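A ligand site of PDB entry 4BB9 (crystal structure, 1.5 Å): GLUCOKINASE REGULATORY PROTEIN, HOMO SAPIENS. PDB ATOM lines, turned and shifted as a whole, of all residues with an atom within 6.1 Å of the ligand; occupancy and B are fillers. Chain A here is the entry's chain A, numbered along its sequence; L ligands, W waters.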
ATOM      1  N   GLY A 107     -21.532  31.050  14.796  1.00  0.00           N
ATOM      2  CA  GLY A 107     -20.610  30.790  13.681  1.00  0.00           C
ATOM      3  C   GLY A 107     -21.237  31.240  12.376  1.00  0.00           C
ATOM      4  O   GLY A 107     -22.470  31.285  12.245  1.00  0.00           O
ATOM      5  N   GLY A 108     -20.405  31.563  11.392  1.00  0.00           N
ATOM      6  CA  GLY A 108     -20.905  31.919  10.066  1.00  0.00           C
ATOM      7  C   GLY A 108     -21.977  33.000  10.063  1.00  0.00           C
ATOM      8  O   GLY A 108     -21.821  34.023  10.746  1.00  0.00           O
ATOM      9  N   THR A 109     -23.082  32.789   9.317  1.00  0.00           N
ATOM     10  CA  THR A 109     -24.134  33.805   9.268  1.00  0.00           C
ATOM     11  C   THR A 109     -24.723  34.059  10.658  1.00  0.00           C
ATOM     12  O   THR A 109     -25.120  35.180  10.950  1.00  0.00           O
ATOM     13  CB  THR A 109     -25.227  33.465   8.235  1.00  0.00           C
ATOM     14  OG1 THR A 109     -24.661  33.493   6.936  1.00  0.00           O
ATOM     15  CG2 THR A 109     -26.384  34.486   8.260  1.00  0.00           C
ATOM     16  N   SER A 110     -24.798  33.015  11.513  1.00  0.00           N
ATOM     17  CA  SER A 110     -25.316  33.250  12.875  1.00  0.00           C
ATOM     18  C   SER A 110     -24.386  34.221  13.646  1.00  0.00           C
ATOM     19  O   SER A 110     -24.882  35.095  14.356  1.00  0.00           O
ATOM     20  CB  SER A 110     -25.467  31.930  13.622  1.00  0.00           C
ATOM     21  OG  SER A 110     -26.591  31.229  13.111  1.00  0.00           O
ATOM     22  N   GLY A 111     -23.060  34.064  13.499  1.00  0.00           N
ATOM     23  CA  GLY A 111     -22.111  34.984  14.093  1.00  0.00           C
ATOM     24  C   GLY A 111     -22.196  36.369  13.478  1.00  0.00           C
ATOM     25  O   GLY A 111     -22.033  37.368  14.188  1.00  0.00           O
ATOM     26  N   ARG A 112     -22.477  36.455  12.147  1.00  0.00           N
ATOM     27  CA  ARG A 112     -22.574  37.772  11.513  1.00  0.00           C
ATOM     28  C   ARG A 112     -23.864  38.458  11.955  1.00  0.00           C
ATOM     29  O   ARG A 112     -23.884  39.673  12.082  1.00  0.00           O
ATOM     30  CB  ARG A 112     -22.451  37.673   9.987  1.00  0.00           C
ATOM     31  CG  ARG A 112     -21.116  37.095   9.560  1.00  0.00           C
ATOM     32  CD  ARG A 112     -20.888  37.130   8.057  1.00  0.00           C
ATOM     33  NE  ARG A 112     -19.724  36.283   7.749  1.00  0.00           N
ATOM     34  CZ  ARG A 112     -19.785  34.993   7.427  1.00  0.00           C
ATOM     35  NH1 ARG A 112     -20.951  34.414   7.179  1.00  0.00           N
ATOM     36  NH2 ARG A 112     -18.658  34.287   7.304  1.00  0.00           N
ATOM     37  N   GLU A 150     -15.521  28.993   8.414  1.00  0.00           N
ATOM     38  CA  GLU A 150     -16.554  28.174   9.055  1.00  0.00           C
ATOM     39  C   GLU A 150     -16.055  27.106  10.008  1.00  0.00           C
ATOM     40  O   GLU A 150     -16.764  26.771  10.960  1.00  0.00           O
ATOM     41  CB  GLU A 150     -17.532  27.575   8.051  1.00  0.00           C
ATOM     42  CG  GLU A 150     -18.377  28.613   7.303  1.00  0.00           C
ATOM     43  CD  GLU A 150     -17.678  29.229   6.101  1.00  0.00           C
ATOM     44  OE1 GLU A 150     -16.554  28.779   5.765  1.00  0.00           O
ATOM     45  OE2 GLU A 150     -18.247  30.168   5.502  1.00  0.00           O
ATOM     46  N   GLU A 153     -15.882  27.299  14.168  1.00  0.00           N
ATOM     47  CA  GLU A 153     -16.950  27.028  15.132  1.00  0.00           C
ATOM     48  C   GLU A 153     -16.895  25.617  15.722  1.00  0.00           C
ATOM     49  O   GLU A 153     -17.719  25.297  16.587  1.00  0.00           O
ATOM     50  CB  GLU A 153     -18.315  27.236  14.506  1.00  0.00           C
ATOM     51  CG  GLU A 153     -18.724  26.158  13.527  1.00  0.00           C
ATOM     52  CD  GLU A 153     -20.019  26.434  12.812  1.00  0.00           C
ATOM     53  OE1 GLU A 153     -20.181  27.553  12.263  1.00  0.00           O
ATOM     54  OE2 GLU A 153     -20.829  25.484  12.688  1.00  0.00           O
ATOM     55  N   ILE A 178     -26.535  31.648  19.085  1.00  0.00           N
ATOM     56  CA  ILE A 178     -27.339  31.449  17.876  1.00  0.00           C
ATOM     57  C   ILE A 178     -26.749  30.321  17.062  1.00  0.00           C
ATOM     58  O   ILE A 178     -25.612  30.426  16.629  1.00  0.00           O
ATOM     59  CB  ILE A 178     -27.343  32.747  17.025  1.00  0.00           C
ATOM     60  CG1 ILE A 178     -27.760  33.975  17.872  1.00  0.00           C
ATOM     61  CG2 ILE A 178     -28.265  32.566  15.790  1.00  0.00           C
ATOM     62  CD1 ILE A 178     -27.431  35.321  17.190  1.00  0.00           C
ATOM     63  N   SER A 179     -27.544  29.285  16.798  1.00  0.00           N
ATOM     64  CA  SER A 179     -27.127  28.194  15.906  1.00  0.00           C
ATOM     65  C   SER A 179     -28.385  27.674  15.265  1.00  0.00           C
ATOM     66  O   SER A 179     -29.152  26.955  15.906  1.00  0.00           O
ATOM     67  CB  SER A 179     -26.417  27.088  16.677  1.00  0.00           C
ATOM     68  OG  SER A 179     -26.005  26.079  15.764  1.00  0.00           O
ATOM     69  N   VAL A 180     -28.615  28.054  13.991  1.00  0.00           N
ATOM     70  CA  VAL A 180     -29.813  27.641  13.275  1.00  0.00           C
ATOM     71  C   VAL A 180     -30.082  26.148  13.389  1.00  0.00           C
ATOM     72  O   VAL A 180     -31.205  25.725  13.686  1.00  0.00           O
ATOM     73  CB  VAL A 180     -29.786  28.124  11.808  1.00  0.00           C
ATOM     74  CG1 VAL A 180     -30.887  27.479  10.982  1.00  0.00           C
ATOM     75  CG2 VAL A 180     -29.869  29.646  11.744  1.00  0.00           C
ATOM     76  N   GLY A 181     -29.034  25.344  13.179  1.00  0.00           N
ATOM     77  CA  GLY A 181     -29.205  23.897  13.204  1.00  0.00           C
ATOM     78  C   GLY A 181     -29.143  23.271  14.580  1.00  0.00           C
ATOM     79  O   GLY A 181     -29.308  22.046  14.681  1.00  0.00           O
ATOM     80  N   LEU A 182     -28.931  24.076  15.634  1.00  0.00           N
ATOM     81  CA  LEU A 182     -28.661  23.575  16.989  1.00  0.00           C
ATOM     82  C   LEU A 182     -27.461  22.630  16.813  1.00  0.00           C
ATOM     83  O   LEU A 182     -27.527  21.412  17.084  1.00  0.00           O
ATOM     84  CB  LEU A 182     -29.870  22.884  17.633  1.00  0.00           C
ATOM     85  CG  LEU A 182     -31.144  23.723  17.790  1.00  0.00           C
ATOM     86  CD1 LEU A 182     -32.166  22.973  18.612  1.00  0.00           C
ATOM     87  CD2 LEU A 182     -30.843  25.061  18.478  1.00  0.00           C
ATOM     88  N   SER A 183     -26.385  23.223  16.280  1.00  0.00           N
ATOM     89  CA  SER A 183     -25.243  22.511  15.774  1.00  0.00           C
ATOM     90  C   SER A 183     -23.876  22.949  16.212  1.00  0.00           C
ATOM     91  O   SER A 183     -23.008  22.093  16.428  1.00  0.00           O
ATOM     92  CB  SER A 183     -25.311  22.601  14.246  1.00  0.00           C
ATOM     93  OG  SER A 183     -24.073  22.418  13.576  1.00  0.00           O
ATOM     94  N   ALA A 184     -23.606  24.234  16.246  1.00  0.00           N
ATOM     95  CA  ALA A 184     -22.258  24.754  16.420  1.00  0.00           C
ATOM     96  C   ALA A 184     -21.618  24.431  17.759  1.00  0.00           C
ATOM     97  O   ALA A 184     -22.080  24.946  18.774  1.00  0.00           O
ATOM     98  CB  ALA A 184     -22.220  26.262  16.170  1.00  0.00           C
ATOM     99  N   VAL A 187     -21.086  27.417  20.134  1.00  0.00           N
ATOM    100  CA  VAL A 187     -22.229  27.856  20.911  1.00  0.00           C
ATOM    101  C   VAL A 187     -22.540  26.841  22.035  1.00  0.00           C
ATOM    102  O   VAL A 187     -22.872  27.269  23.140  1.00  0.00           O
ATOM    103  CB  VAL A 187     -23.442  28.056  19.961  1.00  0.00           C
ATOM    104  CG1 VAL A 187     -24.749  28.209  20.745  1.00  0.00           C
ATOM    105  CG2 VAL A 187     -23.215  29.252  19.044  1.00  0.00           C
ATOM    106  N   GLY A 256     -30.500  23.078   3.739  1.00  0.00           N
ATOM    107  CA  GLY A 256     -29.430  23.412   4.658  1.00  0.00           C
ATOM    108  C   GLY A 256     -28.893  24.825   4.534  1.00  0.00           C
ATOM    109  O   GLY A 256     -27.949  25.169   5.234  1.00  0.00           O
ATOM    110  N   SER A 258     -28.968  27.721   5.817  1.00  0.00           N
ATOM    111  CA  SER A 258     -29.356  28.390   7.046  1.00  0.00           C
ATOM    112  C   SER A 258     -29.259  29.906   6.973  1.00  0.00           C
ATOM    113  O   SER A 258     -29.928  30.588   7.751  1.00  0.00           O
ATOM    114  CB  SER A 258     -28.534  27.858   8.213  1.00  0.00           C
ATOM    115  OG  SER A 258     -27.145  28.069   7.991  1.00  0.00           O
ATOM    116  N   ARG A 259     -28.450  30.446   6.032  1.00  0.00           N
ATOM    117  CA  ARG A 259     -28.321  31.899   5.883  1.00  0.00           C
ATOM    118  C   ARG A 259     -29.636  32.538   5.440  1.00  0.00           C
ATOM    119  O   ARG A 259     -29.800  33.753   5.618  1.00  0.00           O
ATOM    120  CB  ARG A 259     -27.226  32.237   4.858  1.00  0.00           C
ATOM    121  CG  ARG A 259     -27.644  32.002   3.390  1.00  0.00           C
ATOM    122  CD  ARG A 259     -26.455  32.140   2.480  1.00  0.00           C
ATOM    123  NE  ARG A 259     -26.794  32.159   1.056  1.00  0.00           N
ATOM    124  CZ  ARG A 259     -26.552  33.181   0.241  1.00  0.00           C
ATOM    125  NH1 ARG A 259     -26.047  34.314   0.718  1.00  0.00           N
ATOM    126  NH2 ARG A 259     -26.834  33.091  -1.050  1.00  0.00           N
ATOM    127  N   GLU A 348     -21.026  33.960   1.936  1.00  0.00           N
ATOM    128  CA  GLU A 348     -21.664  32.650   1.985  1.00  0.00           C
ATOM    129  C   GLU A 348     -21.625  31.895   0.670  1.00  0.00           C
ATOM    130  O   GLU A 348     -21.794  30.664   0.660  1.00  0.00           O
ATOM    131  CB  GLU A 348     -23.079  32.744   2.532  1.00  0.00           C
ATOM    132  CG  GLU A 348     -23.113  33.004   4.032  1.00  0.00           C
ATOM    133  CD  GLU A 348     -22.592  31.890   4.931  1.00  0.00           C
ATOM    134  OE1 GLU A 348     -21.557  31.272   4.610  1.00  0.00           O
ATOM    135  OE2 GLU A 348     -23.172  31.706   6.019  1.00  0.00           O
ATOM    136  N   HIS A 351     -18.694  28.754   0.498  1.00  0.00           N
ATOM    137  CA  HIS A 351     -18.963  27.374   0.846  1.00  0.00           C
ATOM    138  C   HIS A 351     -20.210  26.828   0.173  1.00  0.00           C
ATOM    139  O   HIS A 351     -20.293  25.618  -0.052  1.00  0.00           O
ATOM    140  CB  HIS A 351     -19.061  27.198   2.393  1.00  0.00           C
ATOM    141  CG  HIS A 351     -20.454  27.360   2.950  1.00  0.00           C
ATOM    142  ND1 HIS A 351     -20.958  28.600   3.288  1.00  0.00           N
ATOM    143  CD2 HIS A 351     -21.431  26.434   3.109  1.00  0.00           C
ATOM    144  CE1 HIS A 351     -22.198  28.391   3.702  1.00  0.00           C
ATOM    145  NE2 HIS A 351     -22.535  27.105   3.613  1.00  0.00           N
ATOM    146  N   THR A 352     -21.229  27.680  -0.044  1.00  0.00           N
ATOM    147  CA  THR A 352     -22.495  27.166  -0.554  1.00  0.00           C
ATOM    148  C   THR A 352     -22.389  26.631  -1.969  1.00  0.00           C
ATOM    149  O   THR A 352     -23.019  25.606  -2.291  1.00  0.00           O
ATOM    150  CB  THR A 352     -23.582  28.257  -0.465  1.00  0.00           C
ATOM    151  OG1 THR A 352     -23.656  28.727   0.884  1.00  0.00           O
ATOM    152  CG2 THR A 352     -24.965  27.727  -0.884  1.00  0.00           C
ATOM    153  N   ASN A 512     -16.842  22.905   7.588  1.00  0.00           N
ATOM    154  CA  ASN A 512     -16.979  22.575   9.004  1.00  0.00           C
ATOM    155  C   ASN A 512     -17.637  21.212   9.166  1.00  0.00           C
ATOM    156  O   ASN A 512     -18.054  20.589   8.168  1.00  0.00           O
ATOM    157  CB  ASN A 512     -17.613  23.680   9.852  1.00  0.00           C
ATOM    158  CG  ASN A 512     -19.069  23.931   9.588  1.00  0.00           C
ATOM    159  OD1 ASN A 512     -19.797  23.086   9.047  1.00  0.00           O
ATOM    160  ND2 ASN A 512     -19.522  25.099  10.012  1.00  0.00           N
ATOM    161  N   LYS A 514     -20.578  20.310  10.402  1.00  0.00           N
ATOM    162  CA  LYS A 514     -21.967  20.237   9.953  1.00  0.00           C
ATOM    163  C   LYS A 514     -21.992  19.972   8.428  1.00  0.00           C
ATOM    164  O   LYS A 514     -22.793  19.162   7.958  1.00  0.00           O
ATOM    165  CB  LYS A 514     -22.706  21.570  10.265  1.00  0.00           C
ATOM    166  CG  LYS A 514     -24.186  21.528   9.845  1.00  0.00           C
ATOM    167  CD  LYS A 514     -24.940  22.834  10.051  1.00  0.00           C
ATOM    168  CE  LYS A 514     -24.446  23.921   9.110  1.00  0.00           C
ATOM    169  NZ  LYS A 514     -25.265  25.162   9.204  1.00  0.00           N
ATOM    170  N   LEU A 515     -21.109  20.649   7.679  1.00  0.00           N
ATOM    171  CA  LEU A 515     -21.063  20.513   6.234  1.00  0.00           C
ATOM    172  C   LEU A 515     -20.507  19.170   5.808  1.00  0.00           C
ATOM    173  O   LEU A 515     -20.970  18.640   4.807  1.00  0.00           O
ATOM    174  CB  LEU A 515     -20.285  21.682   5.615  1.00  0.00           C
ATOM    175  CG  LEU A 515     -20.900  23.053   5.909  1.00  0.00           C
ATOM    176  CD1 LEU A 515     -19.976  24.175   5.476  1.00  0.00           C
ATOM    177  CD2 LEU A 515     -22.285  23.206   5.245  1.00  0.00           C
ATOM    178  N   ARG A 518     -23.408  16.904   6.023  1.00  0.00           N
ATOM    179  CA  ARG A 518     -24.328  17.179   4.931  1.00  0.00           C
ATOM    180  C   ARG A 518     -23.807  16.502   3.649  1.00  0.00           C
ATOM    181  O   ARG A 518     -24.596  15.957   2.887  1.00  0.00           O
ATOM    182  CB  ARG A 518     -24.435  18.687   4.742  1.00  0.00           C
ATOM    183  CG  ARG A 518     -25.407  19.097   3.631  1.00  0.00           C
ATOM    184  CD  ARG A 518     -25.547  20.600   3.490  1.00  0.00           C
ATOM    185  NE  ARG A 518     -26.030  21.200   4.735  1.00  0.00           N
ATOM    186  CZ  ARG A 518     -25.985  22.497   5.007  1.00  0.00           C
ATOM    187  NH1 ARG A 518     -25.534  23.360   4.097  1.00  0.00           N
ATOM    188  NH2 ARG A 518     -26.381  22.949   6.191  1.00  0.00           N
HETATM  189  C1  LIG L   1     -23.435  27.985  11.237  1.00  0.00           C
HETATM  190  C2  LIG L   1     -22.680  27.939   9.902  1.00  0.00           C
HETATM  191  C3  LIG L   1     -23.521  28.630   8.843  1.00  0.00           C
HETATM  192  C4  LIG L   1     -22.845  28.570   7.481  1.00  0.00           C
HETATM  193  C5  LIG L   1     -22.688  27.109   7.083  1.00  0.00           C
HETATM  194  C6  LIG L   1     -21.766  26.451   8.173  1.00  0.00           C
HETATM  195  O1  LIG L   1     -24.646  27.243  11.108  1.00  0.00           O
HETATM  196  O2  LIG L   1     -21.443  28.617  10.056  1.00  0.00           O
HETATM  197  O3  LIG L   1     -23.819  29.994   9.179  1.00  0.00           O
HETATM  198  O4  LIG L   1     -23.714  29.167   6.469  1.00  0.00           O
HETATM  199  O5  LIG L   1     -23.953  26.391   7.024  1.00  0.00           O
HETATM  200  O6  LIG L   1     -22.476  26.589   9.481  1.00  0.00           O
HETATM  201  P1  LIG L   1     -25.676  27.282  12.332  1.00  0.00           P
HETATM  202  O7  LIG L   1     -26.698  26.196  11.976  1.00  0.00           O
HETATM  203  O8  LIG L   1     -26.328  28.688  12.427  1.00  0.00           O
HETATM  204  O9  LIG L   1     -24.869  27.038  13.632  1.00  0.00           O
HETATM  205  O   HOH W   1     -26.074  28.766   5.280  1.00  0.00           O
HETATM  206  O   HOH W   2     -24.915  26.123   4.475  1.00  0.00           O
HETATM  207  O   HOH W   3     -26.392  29.840   9.920  1.00  0.00           O
HETATM  208  O   HOH W   4     -23.663  29.193  15.041  1.00  0.00           O
HETATM  209  O   HOH W   5     -23.329  24.820  12.852  1.00  0.00           O
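OG of Ser 110 sits at hydrogen-bond distance from O8 of the ligand (2.6 Å). NZ of Lys 514 lies within salt-bridge range of O7 of the ligand. An oxygen (O8) of the ligand sits at hydrogen-bond distance from the backbone NH (N) of Val 180, 2.8 Å away. An oxygen (O6) of the ligand sits close to the side-chain amide nitrogen (ND2) of Asn 512 (3.4 Å). An oxygen (O3) of the ligand sits at hydrogen-bond distance from the backbone NH of Thr 109 (2.9 Å). O2 of the ligand is in hydrogen-bond range of OE1 of Glu 153, at 2.8 Å. N of Gly 181 sits at hydrogen-bond distance from O7 of the ligand (2.8 Å). An oxygen (O4) of the ligand lies within hydrogen-bond range of the side-chain carboxylate (OE2) of Glu 348, at 2.6 Å. OG of Ser 179 lies within hydrogen-bond range of O9 of the ligand (2.6 Å). An oxygen (O2) of the ligand lies close to the backbone NH (N) of Gly 108, 3.4 Å away.
ND2 of Asn 512 lies within hydrogen-bond range of O of Glu 150 (3.4 Å). The side-chain carboxylate (OE2) of Glu 153 lies within hydrogen-bond range of the side-chain amide nitrogen (ND2) of Asn 512 (3.0 Å). N of Ser 183 lies within hydrogen-bond range of OG of Ser 179, at 2.9 Å. The backbone carbonyl oxygen (O) of Glu 348 sits at hydrogen-bond distance from the side-chain hydroxyl (OG1) of Thr 352 (2.7 Å). OE2 of Glu 348 lies within hydrogen-bond range of OG1 of Thr 109, 2.5 Å away. ND1 of His 351 lies within hydrogen-bond range of OE1 of Glu 348. NE2 of His 351 sits close to OG1 of Thr 352, 3.4 Å away. The side-chain amide oxygen (OD1) of Asn 512 is in hydrogen-bond range of the backbone NH (N) of Lys 514, 3.2 Å away.
Merely in contact with the ligand: His 351 (3.2 Å), Gly 107 (3.5 Å), Ser 258 (3.7 Å), Ala 184 (3.7 Å) and Leu 515 (3.96 Å). Hydrophobic or aromatic side chains that line the ligand: Val 180, Ala 184, His 351 and Leu 515.
Water W1 lies within hydrogen-bond range of O4 of the ligand (2.7 Å), OG of Ser 258 (3.0 Å) and N of Arg 259 (3.0 Å). Water W3 lies within hydrogen-bond range of an oxygen (O3) of the ligand (2.7 Å), the side-chain hydroxyl of Ser 258 (2.7 Å) and the side-chain hydroxyl of Ser 110 (3.5 Å). Water W2 lies within hydrogen-bond range of a ring nitrogen (NE2) of His 351 (2.7 Å), an oxygen (O5) of the ligand (2.7 Å), the guanidinium group of Arg 518 (2.9 Å) and the backbone carbonyl oxygen of Gly 256 (3.3 Å). Water W5 lies within hydrogen-bond range of OE2 of Glu 153 (2.6 Å), OG of Ser 183 (2.6 Å), O9 of the ligand (2.8 Å) and N of Ala 184 (3.5 Å). Water W4 lies within hydrogen-bond range of the backbone carbonyl oxygen of Ile 178 (2.8 Å), the backbone NH of Gly 107 (2.8 Å) and an oxygen (O9) of the ligand (2.8 Å).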
